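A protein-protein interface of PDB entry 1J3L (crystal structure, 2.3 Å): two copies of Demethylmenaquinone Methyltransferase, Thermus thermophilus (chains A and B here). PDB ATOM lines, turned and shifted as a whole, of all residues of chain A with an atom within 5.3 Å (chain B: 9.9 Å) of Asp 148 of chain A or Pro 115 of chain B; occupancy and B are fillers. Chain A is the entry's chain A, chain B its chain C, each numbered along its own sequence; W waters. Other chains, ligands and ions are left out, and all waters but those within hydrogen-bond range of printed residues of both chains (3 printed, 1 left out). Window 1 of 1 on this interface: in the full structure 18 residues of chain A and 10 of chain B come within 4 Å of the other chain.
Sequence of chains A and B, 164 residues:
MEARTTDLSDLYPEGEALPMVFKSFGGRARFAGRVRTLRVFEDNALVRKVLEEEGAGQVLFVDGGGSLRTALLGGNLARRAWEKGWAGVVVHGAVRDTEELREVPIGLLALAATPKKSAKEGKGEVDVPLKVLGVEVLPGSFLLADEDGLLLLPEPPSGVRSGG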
ATOM      1  N   ARG A   4     -29.010  29.050  27.775  1.00  0.00           N
ATOM      2  CA  ARG A   4     -27.976  28.088  27.611  1.00  0.00           C
ATOM      3  C   ARG A   4     -26.724  28.584  28.254  1.00  0.00           C
ATOM      4  O   ARG A   4     -26.483  29.797  28.428  1.00  0.00           O
ATOM      5  CB  ARG A   4     -27.624  27.825  26.169  1.00  0.00           C
ATOM      6  CG  ARG A   4     -28.403  26.721  25.528  1.00  0.00           C
ATOM      7  CD  ARG A   4     -28.387  25.397  26.291  1.00  0.00           C
ATOM      8  NE  ARG A   4     -27.836  24.274  25.524  1.00  0.00           N
ATOM      9  CZ  ARG A   4     -28.065  24.037  24.233  1.00  0.00           C
ATOM     10  NH1 ARG A   4     -28.840  24.845  23.521  1.00  0.00           N
ATOM     11  NH2 ARG A   4     -27.503  22.989  23.644  1.00  0.00           N
ATOM     12  N   THR A   5     -25.882  27.613  28.540  1.00  0.00           N
ATOM     13  CA  THR A   5     -24.644  27.861  29.189  1.00  0.00           C
ATOM     14  C   THR A   5     -23.741  28.492  28.137  1.00  0.00           C
ATOM     15  O   THR A   5     -23.081  29.472  28.440  1.00  0.00           O
ATOM     16  CB  THR A   5     -24.144  26.499  29.756  1.00  0.00           C
ATOM     17  OG1 THR A   5     -23.335  26.698  30.921  1.00  0.00           O
ATOM     18  CG2 THR A   5     -23.413  25.734  28.679  1.00  0.00           C
ATOM     19  N   THR A   6     -23.716  27.920  26.929  1.00  0.00           N
ATOM     20  CA  THR A   6     -22.871  28.400  25.853  1.00  0.00           C
ATOM     21  C   THR A   6     -23.195  29.844  25.450  1.00  0.00           C
ATOM     22  O   THR A   6     -22.354  30.730  25.578  1.00  0.00           O
ATOM     23  CB  THR A   6     -22.959  27.438  24.635  1.00  0.00           C
ATOM     24  OG1 THR A   6     -24.327  27.251  24.256  1.00  0.00           O
ATOM     25  CG2 THR A   6     -22.363  26.091  24.992  1.00  0.00           C
ATOM     26  N   SER A   9     -22.367  32.273  27.857  1.00  0.00           N
ATOM     27  CA  SER A   9     -20.931  32.348  28.091  1.00  0.00           C
ATOM     28  C   SER A   9     -20.356  33.383  27.128  1.00  0.00           C
ATOM     29  O   SER A   9     -19.429  34.117  27.476  1.00  0.00           O
ATOM     30  CB  SER A   9     -20.260  30.998  27.856  1.00  0.00           C
ATOM     31  OG  SER A   9     -18.873  31.088  28.130  1.00  0.00           O
ATOM     32  N   ALA A  17     -16.842  29.099  34.256  1.00  0.00           N
ATOM     33  CA  ALA A  17     -17.465  27.905  33.702  1.00  0.00           C
ATOM     34  C   ALA A  17     -16.749  26.614  34.103  1.00  0.00           C
ATOM     35  O   ALA A  17     -15.528  26.584  34.292  1.00  0.00           O
ATOM     36  CB  ALA A  17     -17.527  28.015  32.174  1.00  0.00           C
ATOM     37  N   LEU A  18     -17.534  25.554  34.249  1.00  0.00           N
ATOM     38  CA  LEU A  18     -17.007  24.246  34.590  1.00  0.00           C
ATOM     39  C   LEU A  18     -17.431  23.269  33.500  1.00  0.00           C
ATOM     40  O   LEU A  18     -18.556  23.338  32.992  1.00  0.00           O
ATOM     41  CB  LEU A  18     -17.542  23.787  35.950  1.00  0.00           C
ATOM     42  CG  LEU A  18     -16.877  24.438  37.164  1.00  0.00           C
ATOM     43  CD1 LEU A  18     -17.568  24.016  38.441  1.00  0.00           C
ATOM     44  CD2 LEU A  18     -15.420  24.037  37.194  1.00  0.00           C
ATOM     45  N   PRO A  19     -16.521  22.370  33.094  1.00  0.00           N
ATOM     46  CA  PRO A  19     -16.863  21.395  32.055  1.00  0.00           C
ATOM     47  C   PRO A  19     -17.883  20.398  32.605  1.00  0.00           C
ATOM     48  O   PRO A  19     -18.019  20.243  33.821  1.00  0.00           O
ATOM     49  CB  PRO A  19     -15.515  20.746  31.732  1.00  0.00           C
ATOM     50  CG  PRO A  19     -14.778  20.844  33.048  1.00  0.00           C
ATOM     51  CD  PRO A  19     -15.118  22.227  33.522  1.00  0.00           C
ATOM     52  N   MET A  20     -18.607  19.741  31.710  1.00  0.00           N
ATOM     53  CA  MET A  20     -19.603  18.764  32.121  1.00  0.00           C
ATOM     54  C   MET A  20     -18.920  17.446  32.475  1.00  0.00           C
ATOM     55  O   MET A  20     -18.996  16.479  31.727  1.00  0.00           O
ATOM     56  CB  MET A  20     -20.638  18.553  31.004  1.00  0.00           C
ATOM     57  CG  MET A  20     -21.786  17.617  31.388  1.00  0.00           C
ATOM     58  SD  MET A  20     -22.267  17.756  33.256  1.00  0.00           S
ATOM     59  CE  MET A  20     -22.912  19.564  33.268  1.00  0.00           C
ATOM     60  N   ASP A 146     -26.508  22.620  32.115  1.00  0.00           N
ATOM     61  CA  ASP A 146     -27.060  21.858  31.003  1.00  0.00           C
ATOM     62  C   ASP A 146     -26.008  20.883  30.469  1.00  0.00           C
ATOM     63  O   ASP A 146     -24.940  20.740  31.060  1.00  0.00           O
ATOM     64  CB  ASP A 146     -27.558  22.796  29.888  1.00  0.00           C
ATOM     65  CG  ASP A 146     -26.454  23.649  29.295  1.00  0.00           C
ATOM     66  OD1 ASP A 146     -25.355  23.114  29.046  1.00  0.00           O
ATOM     67  OD2 ASP A 146     -26.692  24.854  29.061  1.00  0.00           O
ATOM     68  N   GLU A 147     -26.316  20.221  29.355  1.00  0.00           N
ATOM     69  CA  GLU A 147     -25.413  19.250  28.742  1.00  0.00           C
ATOM     70  C   GLU A 147     -24.016  19.759  28.382  1.00  0.00           C
ATOM     71  O   GLU A 147     -23.101  18.960  28.203  1.00  0.00           O
ATOM     72  CB  GLU A 147     -26.046  18.658  27.482  1.00  0.00           C
ATOM     73  CG  GLU A 147     -26.213  19.644  26.336  1.00  0.00           C
ATOM     74  CD  GLU A 147     -27.541  20.393  26.370  1.00  0.00           C
ATOM     75  OE1 GLU A 147     -28.332  20.192  27.318  1.00  0.00           O
ATOM     76  OE2 GLU A 147     -27.793  21.185  25.436  1.00  0.00           O
ATOM     77  N   ASP A 148     -23.843  21.072  28.262  1.00  0.00           N
ATOM     78  CA  ASP A 148     -22.533  21.608  27.917  1.00  0.00           C
ATOM     79  C   ASP A 148     -21.745  22.037  29.142  1.00  0.00           C
ATOM     80  O   ASP A 148     -20.627  22.535  29.016  1.00  0.00           O
ATOM     81  CB  ASP A 148     -22.652  22.799  26.955  1.00  0.00           C
ATOM     82  CG  ASP A 148     -23.268  22.419  25.618  1.00  0.00           C
ATOM     83  OD1 ASP A 148     -22.757  21.481  24.968  1.00  0.00           O
ATOM     84  OD2 ASP A 148     -24.259  23.067  25.217  1.00  0.00           O
ATOM     85  N   GLY A 149     -22.324  21.861  30.325  1.00  0.00           N
ATOM     86  CA  GLY A 149     -21.611  22.245  31.528  1.00  0.00           C
ATOM     87  C   GLY A 149     -22.318  23.215  32.458  1.00  0.00           C
ATOM     88  O   GLY A 149     -23.539  23.359  32.422  1.00  0.00           O
ATOM     89  N   LEU A 150     -21.532  23.885  33.294  1.00  0.00           N
ATOM     90  CA  LEU A 150     -22.061  24.827  34.276  1.00  0.00           C
ATOM     91  C   LEU A 150     -21.516  26.232  34.091  1.00  0.00           C
ATOM     92  O   LEU A 150     -20.305  26.426  33.983  1.00  0.00           O
ATOM     93  CB  LEU A 150     -21.702  24.369  35.689  1.00  0.00           C
ATOM     94  CG  LEU A 150     -21.856  22.891  36.050  1.00  0.00           C
ATOM     95  CD1 LEU A 150     -21.385  22.668  37.480  1.00  0.00           C
ATOM     96  CD2 LEU A 150     -23.292  22.480  35.903  1.00  0.00           C
ATOM     97  N   LEU A 151     -22.414  27.213  34.068  1.00  0.00           N
ATOM     98  CA  LEU A 151     -22.013  28.605  33.932  1.00  0.00           C
ATOM     99  C   LEU A 151     -22.369  29.355  35.217  1.00  0.00           C
ATOM    100  O   LEU A 151     -23.504  29.295  35.692  1.00  0.00           O
ATOM    101  CB  LEU A 151     -22.719  29.261  32.743  1.00  0.00           C
ATOM    102  CG  LEU A 151     -22.277  30.700  32.427  1.00  0.00           C
ATOM    103  CD1 LEU A 151     -20.826  30.706  31.970  1.00  0.00           C
ATOM    104  CD2 LEU A 151     -23.163  31.295  31.348  1.00  0.00           C
ATOM    105  N   PHE B  25     -19.373  12.509  20.430  1.00  0.00           N
ATOM    106  CA  PHE B  25     -20.379  13.548  20.304  1.00  0.00           C
ATOM    107  C   PHE B  25     -21.073  13.590  18.932  1.00  0.00           C
ATOM    108  O   PHE B  25     -22.226  14.053  18.812  1.00  0.00           O
ATOM    109  CB  PHE B  25     -19.712  14.893  20.589  1.00  0.00           C
ATOM    110  CG  PHE B  25     -19.416  15.127  22.035  1.00  0.00           C
ATOM    111  CD1 PHE B  25     -20.425  15.528  22.905  1.00  0.00           C
ATOM    112  CD2 PHE B  25     -18.126  14.992  22.519  1.00  0.00           C
ATOM    113  CE1 PHE B  25     -20.163  15.794  24.237  1.00  0.00           C
ATOM    114  CE2 PHE B  25     -17.845  15.255  23.863  1.00  0.00           C
ATOM    115  CZ  PHE B  25     -18.871  15.664  24.721  1.00  0.00           C
ATOM    116  N   SER B  67      -7.036  20.204  27.880  1.00  0.00           N
ATOM    117  CA  SER B  67      -7.728  21.209  28.674  1.00  0.00           C
ATOM    118  C   SER B  67      -9.243  21.175  28.490  1.00  0.00           C
ATOM    119  O   SER B  67      -9.747  21.007  27.378  1.00  0.00           O
ATOM    120  CB  SER B  67      -7.212  22.609  28.344  1.00  0.00           C
ATOM    121  OG  SER B  67      -7.981  23.590  29.019  1.00  0.00           O
ATOM    122  N   LEU B  68      -9.967  21.343  29.594  1.00  0.00           N
ATOM    123  CA  LEU B  68     -11.419  21.340  29.547  1.00  0.00           C
ATOM    124  C   LEU B  68     -11.962  22.740  29.804  1.00  0.00           C
ATOM    125  O   LEU B  68     -13.169  22.927  29.928  1.00  0.00           O
ATOM    126  CB  LEU B  68     -11.981  20.373  30.594  1.00  0.00           C
ATOM    127  CG  LEU B  68     -11.402  18.955  30.598  1.00  0.00           C
ATOM    128  CD1 LEU B  68     -12.101  18.127  31.677  1.00  0.00           C
ATOM    129  CD2 LEU B  68     -11.565  18.318  29.225  1.00  0.00           C
ATOM    130  N   ARG B  69     -11.065  23.719  29.873  1.00  0.00           N
ATOM    131  CA  ARG B  69     -11.448  25.103  30.143  1.00  0.00           C
ATOM    132  C   ARG B  69     -12.202  25.769  29.007  1.00  0.00           C
ATOM    133  O   ARG B  69     -13.072  26.602  29.241  1.00  0.00           O
ATOM    134  CB  ARG B  69     -10.215  25.946  30.450  1.00  0.00           C
ATOM    135  CG  ARG B  69      -9.516  25.654  31.753  1.00  0.00           C
ATOM    136  CD  ARG B  69      -8.345  26.605  31.850  1.00  0.00           C
ATOM    137  NE  ARG B  69      -7.725  26.614  33.163  1.00  0.00           N
ATOM    138  CZ  ARG B  69      -6.718  27.414  33.486  1.00  0.00           C
ATOM    139  NH1 ARG B  69      -6.239  28.257  32.581  1.00  0.00           N
ATOM    140  NH2 ARG B  69      -6.199  27.372  34.704  1.00  0.00           N
ATOM    141  N   THR B  70     -11.848  25.429  27.772  1.00  0.00           N
ATOM    142  CA  THR B  70     -12.525  26.019  26.622  1.00  0.00           C
ATOM    143  C   THR B  70     -12.783  24.991  25.538  1.00  0.00           C
ATOM    144  O   THR B  70     -12.088  23.980  25.449  1.00  0.00           O
ATOM    145  CB  THR B  70     -11.707  27.168  25.994  1.00  0.00           C
ATOM    146  OG1 THR B  70     -10.482  26.648  25.466  1.00  0.00           O
ATOM    147  CG2 THR B  70     -11.396  28.240  27.034  1.00  0.00           C
ATOM    148  N   ALA B  71     -13.791  25.258  24.719  1.00  0.00           N
ATOM    149  CA  ALA B  71     -14.144  24.380  23.621  1.00  0.00           C
ATOM    150  C   ALA B  71     -13.381  24.778  22.337  1.00  0.00           C
ATOM    151  O   ALA B  71     -13.388  25.936  21.911  1.00  0.00           O
ATOM    152  CB  ALA B  71     -15.644  24.429  23.391  1.00  0.00           C
ATOM    153  N   LEU B  72     -12.721  23.802  21.729  1.00  0.00           N
ATOM    154  CA  LEU B  72     -11.953  24.025  20.519  1.00  0.00           C
ATOM    155  C   LEU B  72     -12.815  23.832  19.287  1.00  0.00           C
ATOM    156  O   LEU B  72     -12.373  24.080  18.167  1.00  0.00           O
ATOM    157  CB  LEU B  72     -10.779  23.047  20.467  1.00  0.00           C
ATOM    158  CG  LEU B  72      -9.786  23.170  21.620  1.00  0.00           C
ATOM    159  CD1 LEU B  72      -8.867  21.969  21.624  1.00  0.00           C
ATOM    160  CD2 LEU B  72      -9.003  24.472  21.485  1.00  0.00           C
ATOM    161  N   LEU B  73     -14.044  23.383  19.493  1.00  0.00           N
ATOM    162  CA  LEU B  73     -14.941  23.149  18.380  1.00  0.00           C
ATOM    163  C   LEU B  73     -16.398  23.137  18.821  1.00  0.00           C
ATOM    164  O   LEU B  73     -16.736  22.646  19.901  1.00  0.00           O
ATOM    165  CB  LEU B  73     -14.555  21.831  17.702  1.00  0.00           C
ATOM    166  CG  LEU B  73     -15.336  21.336  16.488  1.00  0.00           C
ATOM    167  CD1 LEU B  73     -14.461  20.403  15.674  1.00  0.00           C
ATOM    168  CD2 LEU B  73     -16.608  20.633  16.951  1.00  0.00           C
ATOM    169  N   GLY B  74     -17.259  23.696  17.977  1.00  0.00           N
ATOM    170  CA  GLY B  74     -18.675  23.749  18.282  1.00  0.00           C
ATOM    171  C   GLY B  74     -19.521  23.250  17.130  1.00  0.00           C
ATOM    172  O   GLY B  74     -19.024  22.565  16.238  1.00  0.00           O
ATOM    173  N   GLY B  75     -20.802  23.594  17.157  1.00  0.00           N
ATOM    174  CA  GLY B  75     -21.706  23.166  16.114  1.00  0.00           C
ATOM    175  C   GLY B  75     -21.361  23.748  14.759  1.00  0.00           C
ATOM    176  O   GLY B  75     -21.269  23.023  13.768  1.00  0.00           O
ATOM    177  N   ALA B  94     -11.745  19.971  24.958  1.00  0.00           N
ATOM    178  CA  ALA B  94     -13.184  20.175  25.055  1.00  0.00           C
ATOM    179  C   ALA B  94     -13.840  20.768  23.805  1.00  0.00           C
ATOM    180  O   ALA B  94     -13.180  21.363  22.955  1.00  0.00           O
ATOM    181  CB  ALA B  94     -13.490  21.051  26.265  1.00  0.00           C
ATOM    182  N   VAL B  95     -15.153  20.579  23.719  1.00  0.00           N
ATOM    183  CA  VAL B  95     -15.976  21.076  22.629  1.00  0.00           C
ATOM    184  C   VAL B  95     -17.298  21.533  23.252  1.00  0.00           C
ATOM    185  O   VAL B  95     -17.477  21.456  24.470  1.00  0.00           O
ATOM    186  CB  VAL B  95     -16.271  19.971  21.610  1.00  0.00           C
ATOM    187  CG1 VAL B  95     -14.973  19.398  21.093  1.00  0.00           C
ATOM    188  CG2 VAL B  95     -17.127  18.881  22.252  1.00  0.00           C
ATOM    189  N   ARG B  96     -18.214  22.022  22.427  1.00  0.00           N
ATOM    190  CA  ARG B  96     -19.507  22.456  22.926  1.00  0.00           C
ATOM    191  C   ARG B  96     -20.623  22.297  21.894  1.00  0.00           C
ATOM    192  O   ARG B  96     -20.385  21.853  20.768  1.00  0.00           O
ATOM    193  CB  ARG B  96     -19.440  23.894  23.433  1.00  0.00           C
ATOM    194  CG  ARG B  96     -19.137  24.951  22.395  1.00  0.00           C
ATOM    195  CD  ARG B  96     -19.254  26.330  23.034  1.00  0.00           C
ATOM    196  NE  ARG B  96     -18.955  27.419  22.113  1.00  0.00           N
ATOM    197  CZ  ARG B  96     -19.051  28.705  22.431  1.00  0.00           C
ATOM    198  NH1 ARG B  96     -19.437  29.061  23.650  1.00  0.00           N
ATOM    199  NH2 ARG B  96     -18.765  29.634  21.532  1.00  0.00           N
ATOM    200  N   ASP B  97     -21.839  22.652  22.295  1.00  0.00           N
ATOM    201  CA  ASP B  97     -23.017  22.514  21.442  1.00  0.00           C
ATOM    202  C   ASP B  97     -23.313  21.022  21.291  1.00  0.00           C
ATOM    203  O   ASP B  97     -23.556  20.527  20.182  1.00  0.00           O
ATOM    204  CB  ASP B  97     -22.788  23.133  20.055  1.00  0.00           C
ATOM    205  CG  ASP B  97     -22.282  24.550  20.126  1.00  0.00           C
ATOM    206  OD1 ASP B  97     -22.621  25.266  21.098  1.00  0.00           O
ATOM    207  OD2 ASP B  97     -21.550  24.948  19.195  1.00  0.00           O
ATOM    208  N   THR B  98     -23.271  20.317  22.418  1.00  0.00           N
ATOM    209  CA  THR B  98     -23.526  18.881  22.467  1.00  0.00           C
ATOM    210  C   THR B  98     -24.720  18.483  21.606  1.00  0.00           C
ATOM    211  O   THR B  98     -24.663  17.519  20.846  1.00  0.00           O
ATOM    212  CB  THR B  98     -23.786  18.427  23.925  1.00  0.00           C
ATOM    213  OG1 THR B  98     -22.548  18.409  24.646  1.00  0.00           O
ATOM    214  CG2 THR B  98     -24.436  17.048  23.967  1.00  0.00           C
ATOM    215  N   GLU B  99     -25.800  19.236  21.727  1.00  0.00           N
ATOM    216  CA  GLU B  99     -27.016  18.973  20.971  1.00  0.00           C
ATOM    217  C   GLU B  99     -26.824  19.089  19.451  1.00  0.00           C
ATOM    218  O   GLU B  99     -27.375  18.294  18.685  1.00  0.00           O
ATOM    219  CB  GLU B  99     -28.102  19.928  21.460  1.00  0.00           C
ATOM    220  CG  GLU B  99     -29.448  19.764  20.818  1.00  0.00           C
ATOM    221  CD  GLU B  99     -30.541  20.317  21.697  1.00  0.00           C
ATOM    222  OE1 GLU B  99     -31.066  19.558  22.538  1.00  0.00           O
ATOM    223  OE2 GLU B  99     -30.859  21.518  21.563  1.00  0.00           O
ATOM    224  N   GLU B 100     -26.037  20.074  19.026  1.00  0.00           N
ATOM    225  CA  GLU B 100     -25.754  20.296  17.609  1.00  0.00           C
ATOM    226  C   GLU B 100     -24.750  19.295  17.038  1.00  0.00           C
ATOM    227  O   GLU B 100     -24.868  18.871  15.895  1.00  0.00           O
ATOM    228  CB  GLU B 100     -25.201  21.701  17.397  1.00  0.00           C
ATOM    229  CG  GLU B 100     -26.228  22.817  17.441  1.00  0.00           C
ATOM    230  CD  GLU B 100     -25.574  24.187  17.456  1.00  0.00           C
ATOM    231  OE1 GLU B 100     -24.771  24.480  16.536  1.00  0.00           O
ATOM    232  OE2 GLU B 100     -25.859  24.967  18.392  1.00  0.00           O
ATOM    233  N   LEU B 101     -23.749  18.934  17.832  1.00  0.00           N
ATOM    234  CA  LEU B 101     -22.736  17.995  17.380  1.00  0.00           C
ATOM    235  C   LEU B 101     -23.337  16.641  16.989  1.00  0.00           C
ATOM    236  O   LEU B 101     -22.992  16.060  15.954  1.00  0.00           O
ATOM    237  CB  LEU B 101     -21.677  17.803  18.476  1.00  0.00           C
ATOM    238  CG  LEU B 101     -20.877  19.027  18.969  1.00  0.00           C
ATOM    239  CD1 LEU B 101     -19.715  18.563  19.832  1.00  0.00           C
ATOM    240  CD2 LEU B 101     -20.333  19.836  17.787  1.00  0.00           C
ATOM    241  N   ARG B 102     -24.245  16.150  17.822  1.00  0.00           N
ATOM    242  CA  ARG B 102     -24.880  14.851  17.604  1.00  0.00           C
ATOM    243  C   ARG B 102     -25.600  14.750  16.265  1.00  0.00           C
ATOM    244  O   ARG B 102     -25.821  13.644  15.757  1.00  0.00           O
ATOM    245  CB  ARG B 102     -25.860  14.551  18.754  1.00  0.00           C
ATOM    246  CG  ARG B 102     -26.616  13.227  18.631  1.00  0.00           C
ATOM    247  CD  ARG B 102     -25.674  12.042  18.434  1.00  0.00           C
ATOM    248  NE  ARG B 102     -26.404  10.799  18.181  1.00  0.00           N
ATOM    249  CZ  ARG B 102     -25.853   9.679  17.719  1.00  0.00           C
ATOM    250  NH1 ARG B 102     -24.554   9.631  17.452  1.00  0.00           N
ATOM    251  NH2 ARG B 102     -26.604   8.602  17.521  1.00  0.00           N
ATOM    252  N   ALA B 112     -14.563  16.091  26.952  1.00  0.00           N
ATOM    253  CA  ALA B 112     -15.774  16.568  27.605  1.00  0.00           C
ATOM    254  C   ALA B 112     -16.356  17.760  26.866  1.00  0.00           C
ATOM    255  O   ALA B 112     -15.748  18.293  25.941  1.00  0.00           O
ATOM    256  CB  ALA B 112     -15.459  16.971  29.032  1.00  0.00           C
ATOM    257  N   ALA B 113     -17.540  18.176  27.289  1.00  0.00           N
ATOM    258  CA  ALA B 113     -18.185  19.332  26.703  1.00  0.00           C
ATOM    259  C   ALA B 113     -17.960  20.442  27.720  1.00  0.00           C
ATOM    260  O   ALA B 113     -17.961  20.188  28.925  1.00  0.00           O
ATOM    261  CB  ALA B 113     -19.663  19.065  26.515  1.00  0.00           C
ATOM    262  N   THR B 114     -17.730  21.661  27.241  1.00  0.00           N
ATOM    263  CA  THR B 114     -17.500  22.791  28.130  1.00  0.00           C
ATOM    264  C   THR B 114     -18.124  24.047  27.533  1.00  0.00           C
ATOM    265  O   THR B 114     -18.075  24.268  26.323  1.00  0.00           O
ATOM    266  CB  THR B 114     -15.994  22.997  28.395  1.00  0.00           C
ATOM    267  OG1 THR B 114     -15.834  23.739  29.606  1.00  0.00           O
ATOM    268  CG2 THR B 114     -15.325  23.749  27.255  1.00  0.00           C
ATOM    269  N   PRO B 115     -18.724  24.891  28.383  1.00  0.00           N
ATOM    270  CA  PRO B 115     -19.389  26.133  27.973  1.00  0.00           C
ATOM    271  C   PRO B 115     -18.618  27.162  27.151  1.00  0.00           C
ATOM    272  O   PRO B 115     -18.943  27.397  25.986  1.00  0.00           O
ATOM    273  CB  PRO B 115     -19.890  26.714  29.301  1.00  0.00           C
ATOM    274  CG  PRO B 115     -20.107  25.478  30.155  1.00  0.00           C
ATOM    275  CD  PRO B 115     -18.863  24.679  29.835  1.00  0.00           C
ATOM    276  N   LYS B 116     -17.607  27.777  27.759  1.00  0.00           N
ATOM    277  CA  LYS B 116     -16.822  28.815  27.093  1.00  0.00           C
ATOM    278  C   LYS B 116     -16.164  28.512  25.758  1.00  0.00           C
ATOM    279  O   LYS B 116     -15.681  27.416  25.497  1.00  0.00           O
ATOM    280  CB  LYS B 116     -15.746  29.360  28.035  1.00  0.00           C
ATOM    281  CG  LYS B 116     -16.290  30.085  29.258  1.00  0.00           C
ATOM    282  CD  LYS B 116     -15.168  30.781  30.003  1.00  0.00           C
ATOM    283  CE  LYS B 116     -15.670  31.495  31.240  1.00  0.00           C
ATOM    284  NZ  LYS B 116     -14.630  32.400  31.812  1.00  0.00           N
ATOM    285  N   LYS B 117     -16.135  29.539  24.925  1.00  0.00           N
ATOM    286  CA  LYS B 117     -15.512  29.488  23.618  1.00  0.00           C
ATOM    287  C   LYS B 117     -14.005  29.691  23.830  1.00  0.00           C
ATOM    288  O   LYS B 117     -13.586  30.294  24.820  1.00  0.00           O
ATOM    289  CB  LYS B 117     -16.073  30.625  22.763  1.00  0.00           C
ATOM    290  CG  LYS B 117     -15.775  32.013  23.342  1.00  0.00           C
ATOM    291  CD  LYS B 117     -16.537  33.125  22.629  1.00  0.00           C
ATOM    292  CE  LYS B 117     -16.454  34.434  23.407  1.00  0.00           C
ATOM    293  NZ  LYS B 117     -17.358  35.486  22.857  1.00  0.00           N
ATOM    294  N   SER B 118     -13.192  29.184  22.911  1.00  0.00           N
ATOM    295  CA  SER B 118     -11.750  29.360  23.005  1.00  0.00           C
ATOM    296  C   SER B 118     -11.387  30.720  22.408  1.00  0.00           C
ATOM    297  O   SER B 118     -12.243  31.417  21.863  1.00  0.00           O
ATOM    298  CB  SER B 118     -11.016  28.256  22.240  1.00  0.00           C
ATOM    299  OG  SER B 118     -11.233  26.995  22.838  1.00  0.00           O
HETATM  300  O   HOH W   1     -24.926  25.272  22.122  1.00  0.00           O
HETATM  301  O   HOH W   2     -17.795  31.771  25.618  1.00  0.00           O
HETATM  302  O   HOH W   3     -18.640  15.831  29.308  1.00  0.00           O
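Water W1 bridges OD1 of Asp 97 of chain B and OG1 of Thr 6 of chain A.
Water W3 bridges O of Met 20 of chain A and N of Ala 113 of chain B.
Water W2 bridges OG of Ser 9 of chain A (2.8 Å) and N of Lys 117 of chain B (2.9 Å).
No position is printed for both chains.
The backbone NH (N) of Thr 5 of chain A lies within hydrogen-bond range of the side-chain carboxylate (OD2) of Asp 146 of chain A (2.9 Å).
The backbone carbonyl oxygen (O) of Lys 116 of chain B is in hydrogen-bond range of the backbone NH (N) of Ala 71 of chain B (3.0 Å).
The backbone carbonyl oxygen (O) of Leu 73 of chain B is in hydrogen-bond range of the backbone NH (N) of Arg 96 of chain B (3.0 Å).
N of Met 20 of chain A sits at hydrogen-bond distance from O of Ala 113 of chain B, at 2.9 Å.
N of Asp 97 of chain B sits at hydrogen-bond distance from OD1 of Asp 148 of chain A, 3.1 Å away.
OD1 of Asp 148 of chain A lies within hydrogen-bond range of N of Thr 98 of chain B.
The backbone carbonyl oxygen (O) of Asp 148 of chain A lies close to the backbone nitrogen (N) of Pro 115 of chain B (3.1 Å).
Among the printed residues, pairs that only touch across the chains: Arg 4 of chain A with Glu 99 of chain B (3.8 Å), Thr 5 of chain A with Pro 115 of chain B (3.5 Å), Thr 6 of chain A with Arg 96 of chain B (3.7 Å), Thr 6 of chain A with Asp 97 of chain B (3.99 Å), Thr 6 of chain A with Pro 115 of chain B (3.8 Å), Ser 9 of chain A with Lys 116 of chain B (3.0 Å), Ala 17 of chain A with Pro 115 of chain B (3.9 Å), Ala 17 of chain A with Lys 116 of chain B (3.8 Å), Leu 18 of chain A with Pro 115 of chain B (3.4 Å), Pro 19 of chain A with Leu 68 of chain B (3.7 Å), Pro 19 of chain A with Ala 113 of chain B (3.5 Å), Pro 19 of chain A with Thr 114 of chain B (3.5 Å), Glu 147 of chain A with Thr 98 of chain B (3.6 Å), Glu 147 of chain A with Ala 113 of chain B (3.8 Å), Asp 148 of chain A with Arg 96 of chain B (3.8 Å), Asp 148 of chain A with Ala 113 of chain B (3.6 Å), Asp 148 of chain A with Thr 114 of chain B (3.3 Å), Gly 149 of chain A with Pro 115 of chain B (3.8 Å) and Leu 150 of chain A with Pro 115 of chain B (3.8 Å).
Hydrophobic or aromatic side chains of chain B that line the printed part of chain A: Leu 68, Ala 113 and Pro 115.
Asp 148 of chain A touches six residues of chain B.
Of chain A, only Thr 5 (3.5 Å), Thr 6 (3.8 Å), Ala 17 (3.9 Å), Leu 18 (3.4 Å), Asp 148 (2.9 Å), Gly 149 (3.8 Å) and Leu 150 (3.8 Å) come within 4 Å of Pro 115 of chain B.
Gly 149 of chain A touches just one residue of chain B: Pro 115.
Of the printed residues of chain A, Leu 68 of chain B touches Pro 19 (3.7 Å).
Printed residues of chain A within 4 Å of Glu 99 of chain B: Arg 4 (3.8 Å).
Printed residues of chain B within 4 Å of Leu 18 of chain A: Pro 115.
Printed residues of chain B within 4 Å of Arg 4 of chain A: Glu 99 (3.8 Å).
Leu 101 of chain B touches none of the printed residues of chain A.
Lys 117 of chain B touches none of the printed residues of chain A.
The nearest residue of chain B that does not touch Asp 148 of chain A is Glu 99 of chain B (5.0 Å).
The nearest residue of chain A that does not touch Pro 115 of chain B is Ser 9 of chain A (4.1 Å).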
